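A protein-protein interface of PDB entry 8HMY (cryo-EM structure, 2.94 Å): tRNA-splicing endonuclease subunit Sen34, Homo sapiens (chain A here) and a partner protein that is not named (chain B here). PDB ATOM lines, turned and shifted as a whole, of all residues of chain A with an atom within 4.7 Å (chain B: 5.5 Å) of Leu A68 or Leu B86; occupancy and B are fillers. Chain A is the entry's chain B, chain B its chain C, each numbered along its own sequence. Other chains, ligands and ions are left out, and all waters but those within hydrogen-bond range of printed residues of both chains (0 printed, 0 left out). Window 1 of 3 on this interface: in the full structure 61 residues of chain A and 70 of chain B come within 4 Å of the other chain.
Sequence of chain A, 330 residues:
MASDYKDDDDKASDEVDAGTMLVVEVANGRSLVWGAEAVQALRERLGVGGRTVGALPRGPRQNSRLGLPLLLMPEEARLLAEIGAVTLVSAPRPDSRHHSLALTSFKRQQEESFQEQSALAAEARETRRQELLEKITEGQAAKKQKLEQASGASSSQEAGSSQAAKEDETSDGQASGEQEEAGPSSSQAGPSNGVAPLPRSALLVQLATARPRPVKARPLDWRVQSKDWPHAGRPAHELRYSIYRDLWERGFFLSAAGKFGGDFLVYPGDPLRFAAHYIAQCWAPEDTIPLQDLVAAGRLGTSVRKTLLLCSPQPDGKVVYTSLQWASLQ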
ATOM      1  N   VAL A  33      21.076  34.384  -4.578  1.00  0.00           N
ATOM      2  CA  VAL A  33      20.812  33.270  -5.479  1.00  0.00           C
ATOM      3  C   VAL A  33      20.538  32.040  -4.626  1.00  0.00           C
ATOM      4  O   VAL A  33      21.296  31.742  -3.697  1.00  0.00           O
ATOM      5  CB  VAL A  33      21.985  33.036  -6.445  1.00  0.00           C
ATOM      6  CG1 VAL A  33      21.529  32.241  -7.640  1.00  0.00           C
ATOM      7  CG2 VAL A  33      22.563  34.361  -6.888  1.00  0.00           C
ATOM      8  N   TRP A  34      19.447  31.341  -4.926  1.00  0.00           N
ATOM      9  CA  TRP A  34      18.990  30.231  -4.106  1.00  0.00           C
ATOM     10  C   TRP A  34      19.125  28.881  -4.789  1.00  0.00           C
ATOM     11  O   TRP A  34      18.825  27.859  -4.168  1.00  0.00           O
ATOM     12  CB  TRP A  34      17.534  30.451  -3.688  1.00  0.00           C
ATOM     13  CG  TRP A  34      17.344  31.640  -2.807  1.00  0.00           C
ATOM     14  CD1 TRP A  34      16.967  32.886  -3.190  1.00  0.00           C
ATOM     15  CD2 TRP A  34      17.523  31.693  -1.390  1.00  0.00           C
ATOM     16  NE1 TRP A  34      16.903  33.716  -2.104  1.00  0.00           N
ATOM     17  CE2 TRP A  34      17.242  33.005  -0.986  1.00  0.00           C
ATOM     18  CE3 TRP A  34      17.896  30.756  -0.425  1.00  0.00           C
ATOM     19  CZ2 TRP A  34      17.316  33.403   0.339  1.00  0.00           C
ATOM     20  CZ3 TRP A  34      17.972  31.154   0.884  1.00  0.00           C
ATOM     21  CH2 TRP A  34      17.683  32.463   1.257  1.00  0.00           C
ATOM     22  N   GLY A  35      19.571  28.844  -6.044  1.00  0.00           N
ATOM     23  CA  GLY A  35      19.767  27.609  -6.764  1.00  0.00           C
ATOM     24  C   GLY A  35      21.239  27.244  -6.863  1.00  0.00           C
ATOM     25  O   GLY A  35      22.128  28.044  -6.592  1.00  0.00           O
ATOM     26  N   ALA A  36      21.480  25.995  -7.256  1.00  0.00           N
ATOM     27  CA  ALA A  36      22.833  25.483  -7.439  1.00  0.00           C
ATOM     28  C   ALA A  36      23.285  25.517  -8.889  1.00  0.00           C
ATOM     29  O   ALA A  36      24.444  25.851  -9.169  1.00  0.00           O
ATOM     30  CB  ALA A  36      22.931  24.052  -6.910  1.00  0.00           C
ATOM     31  N   VAL A  39      24.423  29.055  -9.608  1.00  0.00           N
ATOM     32  CA  VAL A  39      25.762  29.405  -9.142  1.00  0.00           C
ATOM     33  C   VAL A  39      26.820  28.742 -10.013  1.00  0.00           C
ATOM     34  O   VAL A  39      27.847  29.351 -10.343  1.00  0.00           O
ATOM     35  CB  VAL A  39      25.936  29.031  -7.660  1.00  0.00           C
ATOM     36  CG1 VAL A  39      27.292  29.488  -7.161  1.00  0.00           C
ATOM     37  CG2 VAL A  39      24.841  29.652  -6.828  1.00  0.00           C
ATOM     38  N   THR A  52      28.949  32.796  -0.246  1.00  0.00           N
ATOM     39  CA  THR A  52      27.917  31.972   0.374  1.00  0.00           C
ATOM     40  C   THR A  52      27.778  32.379   1.836  1.00  0.00           C
ATOM     41  O   THR A  52      28.751  32.321   2.594  1.00  0.00           O
ATOM     42  CB  THR A  52      28.254  30.489   0.262  1.00  0.00           C
ATOM     43  OG1 THR A  52      29.603  30.274   0.682  1.00  0.00           O
ATOM     44  CG2 THR A  52      28.098  30.011  -1.161  1.00  0.00           C
ATOM     45  N   GLY A  54      24.847  31.344   3.750  1.00  0.00           N
ATOM     46  CA  GLY A  54      23.906  30.491   4.442  1.00  0.00           C
ATOM     47  C   GLY A  54      24.559  29.545   5.424  1.00  0.00           C
ATOM     48  O   GLY A  54      25.666  29.800   5.902  1.00  0.00           O
ATOM     49  N   ALA A  55      23.874  28.454   5.745  1.00  0.00           N
ATOM     50  CA  ALA A  55      24.410  27.399   6.585  1.00  0.00           C
ATOM     51  C   ALA A  55      24.463  26.108   5.781  1.00  0.00           C
ATOM     52  O   ALA A  55      23.953  26.025   4.662  1.00  0.00           O
ATOM     53  CB  ALA A  55      23.568  27.215   7.850  1.00  0.00           C
ATOM     54  N   LEU A  66      30.204  27.266   4.340  1.00  0.00           N
ATOM     55  CA  LEU A  66      28.816  27.703   4.366  1.00  0.00           C
ATOM     56  C   LEU A  66      28.143  27.349   3.048  1.00  0.00           C
ATOM     57  O   LEU A  66      28.793  26.950   2.081  1.00  0.00           O
ATOM     58  CB  LEU A  66      28.718  29.206   4.645  1.00  0.00           C
ATOM     59  CG  LEU A  66      29.210  29.646   6.022  1.00  0.00           C
ATOM     60  CD1 LEU A  66      28.971  31.121   6.227  1.00  0.00           C
ATOM     61  CD2 LEU A  66      28.545  28.844   7.118  1.00  0.00           C
ATOM     62  N   GLY A  67      26.822  27.497   3.015  1.00  0.00           N
ATOM     63  CA  GLY A  67      26.051  27.109   1.852  1.00  0.00           C
ATOM     64  C   GLY A  67      25.170  28.207   1.296  1.00  0.00           C
ATOM     65  O   GLY A  67      25.407  29.388   1.556  1.00  0.00           O
ATOM     66  N   LEU A  68      24.143  27.828   0.538  1.00  0.00           N
ATOM     67  CA  LEU A  68      23.284  28.806  -0.109  1.00  0.00           C
ATOM     68  C   LEU A  68      22.447  29.554   0.929  1.00  0.00           C
ATOM     69  O   LEU A  68      22.121  29.005   1.982  1.00  0.00           O
ATOM     70  CB  LEU A  68      22.376  28.118  -1.118  1.00  0.00           C
ATOM     71  CG  LEU A  68      23.111  27.509  -2.306  1.00  0.00           C
ATOM     72  CD1 LEU A  68      22.168  26.690  -3.147  1.00  0.00           C
ATOM     73  CD2 LEU A  68      23.762  28.588  -3.132  1.00  0.00           C
ATOM     74  N   PRO A  69      22.066  30.813   0.650  1.00  0.00           N
ATOM     75  CA  PRO A  69      22.171  31.588  -0.589  1.00  0.00           C
ATOM     76  C   PRO A  69      23.548  32.166  -0.885  1.00  0.00           C
ATOM     77  O   PRO A  69      24.396  32.256  -0.001  1.00  0.00           O
ATOM     78  CB  PRO A  69      21.184  32.721  -0.350  1.00  0.00           C
ATOM     79  CG  PRO A  69      21.327  32.984   1.087  1.00  0.00           C
ATOM     80  CD  PRO A  69      21.482  31.630   1.726  1.00  0.00           C
ATOM     81  N   LEU A  70      23.747  32.567  -2.134  1.00  0.00           N
ATOM     82  CA  LEU A  70      24.956  33.250  -2.570  1.00  0.00           C
ATOM     83  C   LEU A  70      24.656  34.737  -2.703  1.00  0.00           C
ATOM     84  O   LEU A  70      23.760  35.126  -3.455  1.00  0.00           O
ATOM     85  CB  LEU A  70      25.447  32.674  -3.896  1.00  0.00           C
ATOM     86  CG  LEU A  70      26.634  33.376  -4.541  1.00  0.00           C
ATOM     87  CD1 LEU A  70      27.915  32.759  -4.044  1.00  0.00           C
ATOM     88  CD2 LEU A  70      26.547  33.274  -6.043  1.00  0.00           C
ATOM     89  N   GLU B  81      33.673  19.303  -6.603  1.00  0.00           N
ATOM     90  CA  GLU B  81      33.295  19.024  -5.222  1.00  0.00           C
ATOM     91  C   GLU B  81      32.370  20.103  -4.669  1.00  0.00           C
ATOM     92  O   GLU B  81      31.464  19.797  -3.879  1.00  0.00           O
ATOM     93  CB  GLU B  81      34.542  18.872  -4.350  1.00  0.00           C
ATOM     94  CG  GLU B  81      34.859  20.068  -3.471  1.00  0.00           C
ATOM     95  CD  GLU B  81      36.243  19.999  -2.871  1.00  0.00           C
ATOM     96  OE1 GLU B  81      36.721  18.880  -2.592  1.00  0.00           O
ATOM     97  OE2 GLU B  81      36.859  21.068  -2.687  1.00  0.00           O
ATOM     98  N   LEU B  82      32.555  21.353  -5.097  1.00  0.00           N
ATOM     99  CA  LEU B  82      31.692  22.439  -4.645  1.00  0.00           C
ATOM    100  C   LEU B  82      30.280  22.282  -5.190  1.00  0.00           C
ATOM    101  O   LEU B  82      29.300  22.399  -4.448  1.00  0.00           O
ATOM    102  CB  LEU B  82      32.279  23.782  -5.070  1.00  0.00           C
ATOM    103  CG  LEU B  82      32.253  24.936  -4.072  1.00  0.00           C
ATOM    104  CD1 LEU B  82      32.151  26.257  -4.807  1.00  0.00           C
ATOM    105  CD2 LEU B  82      31.126  24.786  -3.078  1.00  0.00           C
ATOM    106  N   TRP B  83      30.154  22.023  -6.491  1.00  0.00           N
ATOM    107  CA  TRP B  83      28.824  21.922  -7.080  1.00  0.00           C
ATOM    108  C   TRP B  83      28.036  20.733  -6.551  1.00  0.00           C
ATOM    109  O   TRP B  83      26.828  20.659  -6.797  1.00  0.00           O
ATOM    110  CB  TRP B  83      28.915  21.852  -8.605  1.00  0.00           C
ATOM    111  CG  TRP B  83      29.755  22.929  -9.245  1.00  0.00           C
ATOM    112  CD1 TRP B  83      30.508  22.799 -10.369  1.00  0.00           C
ATOM    113  CD2 TRP B  83      29.912  24.293  -8.818  1.00  0.00           C
ATOM    114  NE1 TRP B  83      31.131  23.981 -10.664  1.00  0.00           N
ATOM    115  CE2 TRP B  83      30.780  24.915  -9.728  1.00  0.00           C
ATOM    116  CE3 TRP B  83      29.404  25.046  -7.755  1.00  0.00           C
ATOM    117  CZ2 TRP B  83      31.155  26.246  -9.608  1.00  0.00           C
ATOM    118  CZ3 TRP B  83      29.784  26.360  -7.635  1.00  0.00           C
ATOM    119  CH2 TRP B  83      30.648  26.948  -8.555  1.00  0.00           C
ATOM    120  N   GLN B  84      28.681  19.808  -5.845  1.00  0.00           N
ATOM    121  CA  GLN B  84      27.984  18.747  -5.133  1.00  0.00           C
ATOM    122  C   GLN B  84      27.733  19.085  -3.676  1.00  0.00           C
ATOM    123  O   GLN B  84      26.752  18.606  -3.103  1.00  0.00           O
ATOM    124  CB  GLN B  84      28.773  17.438  -5.205  1.00  0.00           C
ATOM    125  CG  GLN B  84      29.047  16.948  -6.609  1.00  0.00           C
ATOM    126  CD  GLN B  84      29.846  15.662  -6.622  1.00  0.00           C
ATOM    127  OE1 GLN B  84      30.076  15.048  -5.579  1.00  0.00           O
ATOM    128  NE2 GLN B  84      30.276  15.243  -7.806  1.00  0.00           N
ATOM    129  N   LEU B  85      28.597  19.893  -3.059  1.00  0.00           N
ATOM    130  CA  LEU B  85      28.353  20.295  -1.679  1.00  0.00           C
ATOM    131  C   LEU B  85      27.154  21.226  -1.556  1.00  0.00           C
ATOM    132  O   LEU B  85      26.437  21.175  -0.553  1.00  0.00           O
ATOM    133  CB  LEU B  85      29.595  20.963  -1.099  1.00  0.00           C
ATOM    134  CG  LEU B  85      29.553  21.349   0.377  1.00  0.00           C
ATOM    135  CD1 LEU B  85      29.922  20.172   1.252  1.00  0.00           C
ATOM    136  CD2 LEU B  85      30.474  22.519   0.635  1.00  0.00           C
ATOM    137  N   LEU B  86      26.911  22.074  -2.555  1.00  0.00           N
ATOM    138  CA  LEU B  86      25.835  23.055  -2.477  1.00  0.00           C
ATOM    139  C   LEU B  86      24.473  22.490  -2.848  1.00  0.00           C
ATOM    140  O   LEU B  86      23.456  23.024  -2.399  1.00  0.00           O
ATOM    141  CB  LEU B  86      26.126  24.251  -3.387  1.00  0.00           C
ATOM    142  CG  LEU B  86      27.319  25.141  -3.052  1.00  0.00           C
ATOM    143  CD1 LEU B  86      27.484  26.190  -4.120  1.00  0.00           C
ATOM    144  CD2 LEU B  86      27.135  25.784  -1.702  1.00  0.00           C
ATOM    145  N   ALA B  87      24.421  21.439  -3.658  1.00  0.00           N
ATOM    146  CA  ALA B  87      23.144  20.846  -4.024  1.00  0.00           C
ATOM    147  C   ALA B  87      22.694  19.852  -2.963  1.00  0.00           C
ATOM    148  O   ALA B  87      22.375  18.702  -3.278  1.00  0.00           O
ATOM    149  CB  ALA B  87      23.239  20.159  -5.387  1.00  0.00           C
ATOM    150  N   GLU B  88      22.661  20.287  -1.708  1.00  0.00           N
ATOM    151  CA  GLU B  88      22.295  19.438  -0.587  1.00  0.00           C
ATOM    152  C   GLU B  88      21.130  20.055   0.169  1.00  0.00           C
ATOM    153  O   GLU B  88      21.124  21.256   0.452  1.00  0.00           O
ATOM    154  CB  GLU B  88      23.476  19.231   0.357  1.00  0.00           C
ATOM    155  CG  GLU B  88      24.461  18.183  -0.111  1.00  0.00           C
ATOM    156  CD  GLU B  88      25.517  17.880   0.927  1.00  0.00           C
ATOM    157  OE1 GLU B  88      26.289  16.917   0.733  1.00  0.00           O
ATOM    158  OE2 GLU B  88      25.576  18.609   1.940  1.00  0.00           O
ATOM    159  N   ARG B  90      18.194  19.763   3.478  1.00  0.00           N
ATOM    160  CA  ARG B  90      17.985  19.275   4.833  1.00  0.00           C
ATOM    161  C   ARG B  90      16.856  18.257   4.846  1.00  0.00           C
ATOM    162  O   ARG B  90      15.755  18.531   4.362  1.00  0.00           O
ATOM    163  CB  ARG B  90      17.667  20.428   5.779  1.00  0.00           C
ATOM    164  CG  ARG B  90      18.693  21.530   5.767  1.00  0.00           C
ATOM    165  CD  ARG B  90      18.067  22.873   6.062  1.00  0.00           C
ATOM    166  NE  ARG B  90      18.756  23.947   5.358  1.00  0.00           N
ATOM    167  CZ  ARG B  90      19.716  24.690   5.889  1.00  0.00           C
ATOM    168  NH1 ARG B  90      20.109  24.473   7.133  1.00  0.00           N
ATOM    169  NH2 ARG B  90      20.289  25.645   5.177  1.00  0.00           N
ATOM    170  N   GLU B 142      16.957  26.918  10.109  1.00  0.00           N
ATOM    171  CA  GLU B 142      18.151  26.535   9.360  1.00  0.00           C
ATOM    172  C   GLU B 142      18.821  25.309   9.972  1.00  0.00           C
ATOM    173  O   GLU B 142      19.204  24.378   9.258  1.00  0.00           O
ATOM    174  CB  GLU B 142      19.130  27.701   9.293  1.00  0.00           C
ATOM    175  CG  GLU B 142      18.735  28.782   8.319  1.00  0.00           C
ATOM    176  CD  GLU B 142      19.856  29.766   8.069  1.00  0.00           C
ATOM    177  OE1 GLU B 142      20.159  30.048   6.890  1.00  0.00           O
ATOM    178  OE2 GLU B 142      20.439  30.259   9.054  1.00  0.00           O
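Arg B90 touches Ala A55 (NH2 to O, 3.7 Å). CD2 of Leu B86 touches CA of Gly A67 (3.9 Å). CD1 of Leu A68 touches O of Leu B86, 3.96 Å away.
The backbone carbonyl oxygen (O) of Gly A67 lies within hydrogen-bond range of the backbone NH (N) of Gly A54, at 3.0 Å.
Of the 10 printed residues of chain B, 2 touch a printed residue of chain A. Printed residues of chain B that touch a printed residue of chain A: Leu B86 and Arg B90. Hydrophobic or aromatic side chains of chain B that line the printed part of chain A: Leu B86. Hydrophobic or aromatic side chains of chain A that line the printed part of chain B: Leu A68. Among the printed residues, no Asp or Glu carboxylate lies within 4 Å of a Lys or Arg side-chain nitrogen of the other chain.
Trp A34 touches none of the printed residues of chain B. Printed residues of chain B within 4 Å of Ala A55: Arg B90. Of the printed residues of chain B, Gly A67 touches Leu B86. Printed residues of chain B within 4 Å of Leu A68: Leu B86. Leu B86 touches just these residues of chain A: Gly A67 (3.9 Å) and Leu A68 (3.96 Å). Of the printed residues of chain A, Arg B90 touches Ala A55 (3.7 Å).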
